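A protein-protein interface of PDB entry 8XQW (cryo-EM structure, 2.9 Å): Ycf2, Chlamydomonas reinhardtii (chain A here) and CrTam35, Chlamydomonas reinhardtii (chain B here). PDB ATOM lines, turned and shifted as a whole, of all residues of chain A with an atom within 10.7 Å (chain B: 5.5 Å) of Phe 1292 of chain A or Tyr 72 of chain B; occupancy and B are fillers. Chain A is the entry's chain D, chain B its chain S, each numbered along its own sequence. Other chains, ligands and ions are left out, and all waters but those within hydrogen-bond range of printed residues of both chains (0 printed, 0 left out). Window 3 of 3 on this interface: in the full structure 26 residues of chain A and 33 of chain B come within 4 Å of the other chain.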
ATOM      1  N   ASN A1290     -20.010  19.272 -21.845  1.00  0.00           N
ATOM      2  CA  ASN A1290     -20.363  20.540 -21.220  1.00  0.00           C
ATOM      3  C   ASN A1290     -20.158  20.469 -19.712  1.00  0.00           C
ATOM      4  O   ASN A1290     -20.628  19.542 -19.060  1.00  0.00           O
ATOM      5  CB  ASN A1290     -21.810  20.910 -21.544  1.00  0.00           C
ATOM      6  CG  ASN A1290     -22.135  22.352 -21.207  1.00  0.00           C
ATOM      7  OD1 ASN A1290     -23.292  22.762 -21.259  1.00  0.00           O
ATOM      8  ND2 ASN A1290     -21.116  23.133 -20.874  1.00  0.00           N
ATOM      9  N   ILE A1291     -19.431  21.447 -19.171  1.00  0.00           N
ATOM     10  CA  ILE A1291     -19.205  21.501 -17.729  1.00  0.00           C
ATOM     11  C   ILE A1291     -19.868  22.738 -17.133  1.00  0.00           C
ATOM     12  O   ILE A1291     -20.366  22.709 -16.000  1.00  0.00           O
ATOM     13  CB  ILE A1291     -17.696  21.454 -17.427  1.00  0.00           C
ATOM     14  CG1 ILE A1291     -17.126  20.068 -17.735  1.00  0.00           C
ATOM     15  CG2 ILE A1291     -17.423  21.819 -15.982  1.00  0.00           C
ATOM     16  CD1 ILE A1291     -16.689  19.872 -19.173  1.00  0.00           C
ATOM     17  N   PHE A1292     -19.882  23.837 -17.889  1.00  0.00           N
ATOM     18  CA  PHE A1292     -20.457  25.089 -17.411  1.00  0.00           C
ATOM     19  C   PHE A1292     -21.906  24.903 -16.972  1.00  0.00           C
ATOM     20  O   PHE A1292     -22.291  25.294 -15.856  1.00  0.00           O
ATOM     21  CB  PHE A1292     -20.352  26.138 -18.517  1.00  0.00           C
ATOM     22  CG  PHE A1292     -20.466  27.547 -18.036  1.00  0.00           C
ATOM     23  CD1 PHE A1292     -19.742  27.978 -16.940  1.00  0.00           C
ATOM     24  CD2 PHE A1292     -21.282  28.450 -18.693  1.00  0.00           C
ATOM     25  CE1 PHE A1292     -19.842  29.279 -16.501  1.00  0.00           C
ATOM     26  CE2 PHE A1292     -21.386  29.752 -18.256  1.00  0.00           C
ATOM     27  CZ  PHE A1292     -20.665  30.168 -17.160  1.00  0.00           C
ATOM     28  N   SER A1293     -22.726  24.313 -17.846  1.00  0.00           N
ATOM     29  CA  SER A1293     -24.122  24.080 -17.500  1.00  0.00           C
ATOM     30  C   SER A1293     -24.236  23.141 -16.311  1.00  0.00           C
ATOM     31  O   SER A1293     -25.113  23.312 -15.461  1.00  0.00           O
ATOM     32  CB  SER A1293     -24.885  23.524 -18.700  1.00  0.00           C
ATOM     33  OG  SER A1293     -24.629  22.143 -18.863  1.00  0.00           O
ATOM     34  N   LYS A1294     -23.345  22.153 -16.224  1.00  0.00           N
ATOM     35  CA  LYS A1294     -23.363  21.254 -15.079  1.00  0.00           C
ATOM     36  C   LYS A1294     -23.183  22.020 -13.776  1.00  0.00           C
ATOM     37  O   LYS A1294     -23.945  21.822 -12.819  1.00  0.00           O
ATOM     38  CB  LYS A1294     -22.272  20.197 -15.226  1.00  0.00           C
ATOM     39  CG  LYS A1294     -22.384  19.377 -16.493  1.00  0.00           C
ATOM     40  CD  LYS A1294     -23.754  18.746 -16.629  1.00  0.00           C
ATOM     41  CE  LYS A1294     -23.965  18.201 -18.026  1.00  0.00           C
ATOM     42  NZ  LYS A1294     -23.964  19.288 -19.039  1.00  0.00           N
ATOM     43  N   LYS A1295     -22.195  22.911 -13.727  1.00  0.00           N
ATOM     44  CA  LYS A1295     -21.913  23.620 -12.486  1.00  0.00           C
ATOM     45  C   LYS A1295     -23.044  24.579 -12.133  1.00  0.00           C
ATOM     46  O   LYS A1295     -23.448  24.679 -10.964  1.00  0.00           O
ATOM     47  CB  LYS A1295     -20.577  24.349 -12.603  1.00  0.00           C
ATOM     48  CG  LYS A1295     -19.429  23.419 -12.967  1.00  0.00           C
ATOM     49  CD  LYS A1295     -18.140  24.171 -13.244  1.00  0.00           C
ATOM     50  CE  LYS A1295     -17.494  24.658 -11.960  1.00  0.00           C
ATOM     51  NZ  LYS A1295     -17.025  23.541 -11.097  1.00  0.00           N
ATOM     52  N   ILE A1296     -23.590  25.280 -13.131  1.00  0.00           N
ATOM     53  CA  ILE A1296     -24.662  26.224 -12.819  1.00  0.00           C
ATOM     54  C   ILE A1296     -25.917  25.476 -12.377  1.00  0.00           C
ATOM     55  O   ILE A1296     -26.639  25.919 -11.470  1.00  0.00           O
ATOM     56  CB  ILE A1296     -24.933  27.167 -14.007  1.00  0.00           C
ATOM     57  CG1 ILE A1296     -25.434  26.407 -15.231  1.00  0.00           C
ATOM     58  CG2 ILE A1296     -23.677  27.934 -14.364  1.00  0.00           C
ATOM     59  CD1 ILE A1296     -25.520  27.261 -16.480  1.00  0.00           C
ATOM     60  N   ILE A1297     -26.176  24.309 -12.973  1.00  0.00           N
ATOM     61  CA  ILE A1297     -27.332  23.515 -12.581  1.00  0.00           C
ATOM     62  C   ILE A1297     -27.162  22.986 -11.163  1.00  0.00           C
ATOM     63  O   ILE A1297     -28.111  22.983 -10.375  1.00  0.00           O
ATOM     64  CB  ILE A1297     -27.555  22.382 -13.599  1.00  0.00           C
ATOM     65  CG1 ILE A1297     -28.094  22.948 -14.913  1.00  0.00           C
ATOM     66  CG2 ILE A1297     -28.515  21.349 -13.059  1.00  0.00           C
ATOM     67  CD1 ILE A1297     -29.383  23.706 -14.759  1.00  0.00           C
ATOM     68  N   SER A1298     -25.953  22.550 -10.807  1.00  0.00           N
ATOM     69  CA  SER A1298     -25.724  22.085  -9.442  1.00  0.00           C
ATOM     70  C   SER A1298     -25.931  23.209  -8.434  1.00  0.00           C
ATOM     71  O   SER A1298     -26.540  23.005  -7.370  1.00  0.00           O
ATOM     72  CB  SER A1298     -24.320  21.502  -9.310  1.00  0.00           C
ATOM     73  OG  SER A1298     -24.299  20.142  -9.703  1.00  0.00           O
ATOM     74  N   LYS A1299     -25.435  24.405  -8.750  1.00  0.00           N
ATOM     75  CA  LYS A1299     -25.631  25.530  -7.843  1.00  0.00           C
ATOM     76  C   LYS A1299     -27.113  25.835  -7.661  1.00  0.00           C
ATOM     77  O   LYS A1299     -27.592  26.003  -6.531  1.00  0.00           O
ATOM     78  CB  LYS A1299     -24.879  26.753  -8.363  1.00  0.00           C
ATOM     79  CG  LYS A1299     -23.360  26.636  -8.271  1.00  0.00           C
ATOM     80  CD  LYS A1299     -22.890  26.606  -6.827  1.00  0.00           C
ATOM     81  CE  LYS A1299     -21.406  26.303  -6.733  1.00  0.00           C
ATOM     82  NZ  LYS A1299     -20.909  26.372  -5.331  1.00  0.00           N
ATOM     83  N   VAL A1300     -27.868  25.891  -8.762  1.00  0.00           N
ATOM     84  CA  VAL A1300     -29.284  26.224  -8.614  1.00  0.00           C
ATOM     85  C   VAL A1300     -30.042  25.101  -7.915  1.00  0.00           C
ATOM     86  O   VAL A1300     -31.032  25.356  -7.221  1.00  0.00           O
ATOM     87  CB  VAL A1300     -29.929  26.584  -9.964  1.00  0.00           C
ATOM     88  CG1 VAL A1300     -29.120  27.647 -10.669  1.00  0.00           C
ATOM     89  CG2 VAL A1300     -30.099  25.353 -10.835  1.00  0.00           C
ATOM     90  N   VAL B  68     -22.778  36.408 -16.457  1.00  0.00           N
ATOM     91  CA  VAL B  68     -21.563  35.605 -16.418  1.00  0.00           C
ATOM     92  C   VAL B  68     -21.401  34.808 -17.700  1.00  0.00           C
ATOM     93  O   VAL B  68     -20.287  34.687 -18.223  1.00  0.00           O
ATOM     94  CB  VAL B  68     -21.585  34.667 -15.200  1.00  0.00           C
ATOM     95  CG1 VAL B  68     -20.417  33.711 -15.242  1.00  0.00           C
ATOM     96  CG2 VAL B  68     -21.565  35.460 -13.921  1.00  0.00           C
ATOM     97  N   ARG B  69     -22.510  34.289 -18.235  1.00  0.00           N
ATOM     98  CA  ARG B  69     -22.455  33.259 -19.265  1.00  0.00           C
ATOM     99  C   ARG B  69     -21.631  33.705 -20.465  1.00  0.00           C
ATOM    100  O   ARG B  69     -20.638  33.060 -20.822  1.00  0.00           O
ATOM    101  CB  ARG B  69     -23.871  32.885 -19.698  1.00  0.00           C
ATOM    102  CG  ARG B  69     -24.542  31.876 -18.790  1.00  0.00           C
ATOM    103  CD  ARG B  69     -25.561  31.048 -19.549  1.00  0.00           C
ATOM    104  NE  ARG B  69     -26.861  31.706 -19.630  1.00  0.00           N
ATOM    105  CZ  ARG B  69     -27.867  31.284 -20.391  1.00  0.00           C
ATOM    106  NH1 ARG B  69     -27.729  30.201 -21.143  1.00  0.00           N
ATOM    107  NH2 ARG B  69     -29.016  31.944 -20.397  1.00  0.00           N
ATOM    108  N   GLN B  70     -22.026  34.810 -21.099  1.00  0.00           N
ATOM    109  CA  GLN B  70     -21.284  35.292 -22.261  1.00  0.00           C
ATOM    110  C   GLN B  70     -19.829  35.576 -21.920  1.00  0.00           C
ATOM    111  O   GLN B  70     -18.944  35.346 -22.751  1.00  0.00           O
ATOM    112  CB  GLN B  70     -21.957  36.538 -22.831  1.00  0.00           C
ATOM    113  CG  GLN B  70     -22.303  37.591 -21.794  1.00  0.00           C
ATOM    114  CD  GLN B  70     -21.250  38.670 -21.670  1.00  0.00           C
ATOM    115  OE1 GLN B  70     -20.091  38.470 -22.026  1.00  0.00           O
ATOM    116  NE2 GLN B  70     -21.654  39.832 -21.173  1.00  0.00           N
ATOM    117  N   ARG B  71     -19.562  36.055 -20.704  1.00  0.00           N
ATOM    118  CA  ARG B  71     -18.193  36.323 -20.287  1.00  0.00           C
ATOM    119  C   ARG B  71     -17.319  35.081 -20.332  1.00  0.00           C
ATOM    120  O   ARG B  71     -16.099  35.200 -20.466  1.00  0.00           O
ATOM    121  CB  ARG B  71     -18.188  36.902 -18.879  1.00  0.00           C
ATOM    122  CG  ARG B  71     -18.375  38.394 -18.833  1.00  0.00           C
ATOM    123  CD  ARG B  71     -17.065  39.053 -18.472  1.00  0.00           C
ATOM    124  NE  ARG B  71     -16.295  38.223 -17.555  1.00  0.00           N
ATOM    125  CZ  ARG B  71     -16.433  38.251 -16.236  1.00  0.00           C
ATOM    126  NH1 ARG B  71     -17.304  39.079 -15.680  1.00  0.00           N
ATOM    127  NH2 ARG B  71     -15.695  37.459 -15.474  1.00  0.00           N
ATOM    128  N   TYR B  72     -17.910  33.896 -20.216  1.00  0.00           N
ATOM    129  CA  TYR B  72     -17.133  32.672 -20.320  1.00  0.00           C
ATOM    130  C   TYR B  72     -16.773  32.337 -21.757  1.00  0.00           C
ATOM    131  O   TYR B  72     -15.749  31.689 -21.996  1.00  0.00           O
ATOM    132  CB  TYR B  72     -17.901  31.504 -19.696  1.00  0.00           C
ATOM    133  CG  TYR B  72     -17.264  30.150 -19.909  1.00  0.00           C
ATOM    134  CD1 TYR B  72     -16.220  29.716 -19.105  1.00  0.00           C
ATOM    135  CD2 TYR B  72     -17.720  29.298 -20.909  1.00  0.00           C
ATOM    136  CE1 TYR B  72     -15.643  28.475 -19.293  1.00  0.00           C
ATOM    137  CE2 TYR B  72     -17.150  28.056 -21.106  1.00  0.00           C
ATOM    138  CZ  TYR B  72     -16.110  27.649 -20.296  1.00  0.00           C
ATOM    139  OH  TYR B  72     -15.538  26.413 -20.489  1.00  0.00           O
ATOM    140  N   ALA B  73     -17.589  32.770 -22.721  1.00  0.00           N
ATOM    141  CA  ALA B  73     -17.271  32.513 -24.121  1.00  0.00           C
ATOM    142  C   ALA B  73     -16.051  33.305 -24.563  1.00  0.00           C
ATOM    143  O   ALA B  73     -15.163  32.768 -25.234  1.00  0.00           O
ATOM    144  CB  ALA B  73     -18.474  32.845 -25.002  1.00  0.00           C
ATOM    145  N   GLU B  74     -15.990  34.584 -24.206  1.00  0.00           N
ATOM    146  CA  GLU B  74     -14.897  35.454 -24.640  1.00  0.00           C
ATOM    147  C   GLU B  74     -13.743  35.510 -23.646  1.00  0.00           C
ATOM    148  O   GLU B  74     -13.248  36.595 -23.337  1.00  0.00           O
ATOM    149  CB  GLU B  74     -15.454  36.848 -24.922  1.00  0.00           C
ATOM    150  CG  GLU B  74     -16.415  37.390 -23.862  1.00  0.00           C
ATOM    151  CD  GLU B  74     -15.871  38.586 -23.096  1.00  0.00           C
ATOM    152  OE1 GLU B  74     -14.643  38.790 -23.076  1.00  0.00           O
ATOM    153  OE2 GLU B  74     -16.684  39.339 -22.519  1.00  0.00           O
ATOM    154  N   GLY B  75     -13.267  34.374 -23.139  1.00  0.00           N
ATOM    155  CA  GLY B  75     -11.989  34.357 -22.447  1.00  0.00           C
ATOM    156  C   GLY B  75     -11.971  35.043 -21.098  1.00  0.00           C
ATOM    157  O   GLY B  75     -11.386  34.539 -20.134  1.00  0.00           O
ATOM    158  N   ILE B  77     -13.354  35.360 -18.479  1.00  0.00           N
ATOM    159  CA  ILE B  77     -14.019  34.952 -17.243  1.00  0.00           C
ATOM    160  C   ILE B  77     -13.013  34.695 -16.120  1.00  0.00           C
ATOM    161  O   ILE B  77     -13.020  35.389 -15.096  1.00  0.00           O
ATOM    162  CB  ILE B  77     -14.947  33.746 -17.499  1.00  0.00           C
ATOM    163  CG1 ILE B  77     -15.781  33.459 -16.252  1.00  0.00           C
ATOM    164  CG2 ILE B  77     -14.200  32.514 -18.036  1.00  0.00           C
ATOM    165  CD1 ILE B  77     -17.077  34.222 -16.217  1.00  0.00           C
ATOM    166  N   LEU B  83     -13.714  31.694 -11.426  1.00  0.00           N
ATOM    167  CA  LEU B  83     -15.043  31.356 -11.906  1.00  0.00           C
ATOM    168  C   LEU B  83     -15.893  30.788 -10.785  1.00  0.00           C
ATOM    169  O   LEU B  83     -17.055  31.157 -10.624  1.00  0.00           O
ATOM    170  CB  LEU B  83     -14.957  30.346 -13.050  1.00  0.00           C
ATOM    171  CG  LEU B  83     -16.274  29.684 -13.444  1.00  0.00           C
ATOM    172  CD1 LEU B  83     -17.155  30.658 -14.201  1.00  0.00           C
ATOM    173  CD2 LEU B  83     -16.016  28.434 -14.261  1.00  0.00           C
ATOM    174  N   LEU B  87     -19.629  32.285  -9.795  1.00  0.00           N
ATOM    175  CA  LEU B  87     -20.961  31.700  -9.797  1.00  0.00           C
ATOM    176  C   LEU B  87     -21.662  31.872  -8.457  1.00  0.00           C
ATOM    177  O   LEU B  87     -22.893  31.932  -8.417  1.00  0.00           O
ATOM    178  CB  LEU B  87     -20.885  30.221 -10.171  1.00  0.00           C
ATOM    179  CG  LEU B  87     -20.532  29.951 -11.633  1.00  0.00           C
ATOM    180  CD1 LEU B  87     -20.283  28.472 -11.874  1.00  0.00           C
ATOM    181  CD2 LEU B  87     -21.633  30.460 -12.536  1.00  0.00           C
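Of the printed residues of chain B, Ile 1296 of chain A touches Leu 87 (3.7 Å).
Ile 1297 of chain A touches none of the printed residues of chain B.
No residue of chain A comes within 4 Å of Val 68 of chain B.
Printed residues of chain A within 4 Å of Arg 69 of chain B: Phe 1292.
Printed residues of chain A within 4 Å of Tyr 72 of chain B: Phe 1292 (3.98 Å).
No residue of chain A comes within 4 Å of Ala 73 of chain B.
Printed residues of chain A within 4 Å of Leu 83 of chain B: Phe 1292 (3.8 Å).
Of the printed residues of chain A, Leu 87 of chain B touches Ile 1296.
Among the printed residues, merely in contact across the chains: Phe 1292 of chain A with Arg 69 of chain B (3.8 Å), Phe 1292 of chain A with Tyr 72 of chain B (3.98 Å), Phe 1292 of chain A with Leu 83 of chain B (3.8 Å) and Ile 1296 of chain A with Leu 87 of chain B (3.7 Å).
The backbone NH (N) of Phe 1292 of chain A lies close to the side-chain amide nitrogen (ND2) of Asn 1290 of chain A (3.3 Å).
Of the 11 printed residues of chain B, 4 touch a printed residue of chain A.
Hydrophobic or aromatic side chains of chain B that line the printed part of chain A: Tyr 72, Leu 83 and Leu 87.
Printed residues of chain A that touch a printed residue of chain B: Phe 1292 and Ile 1296.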
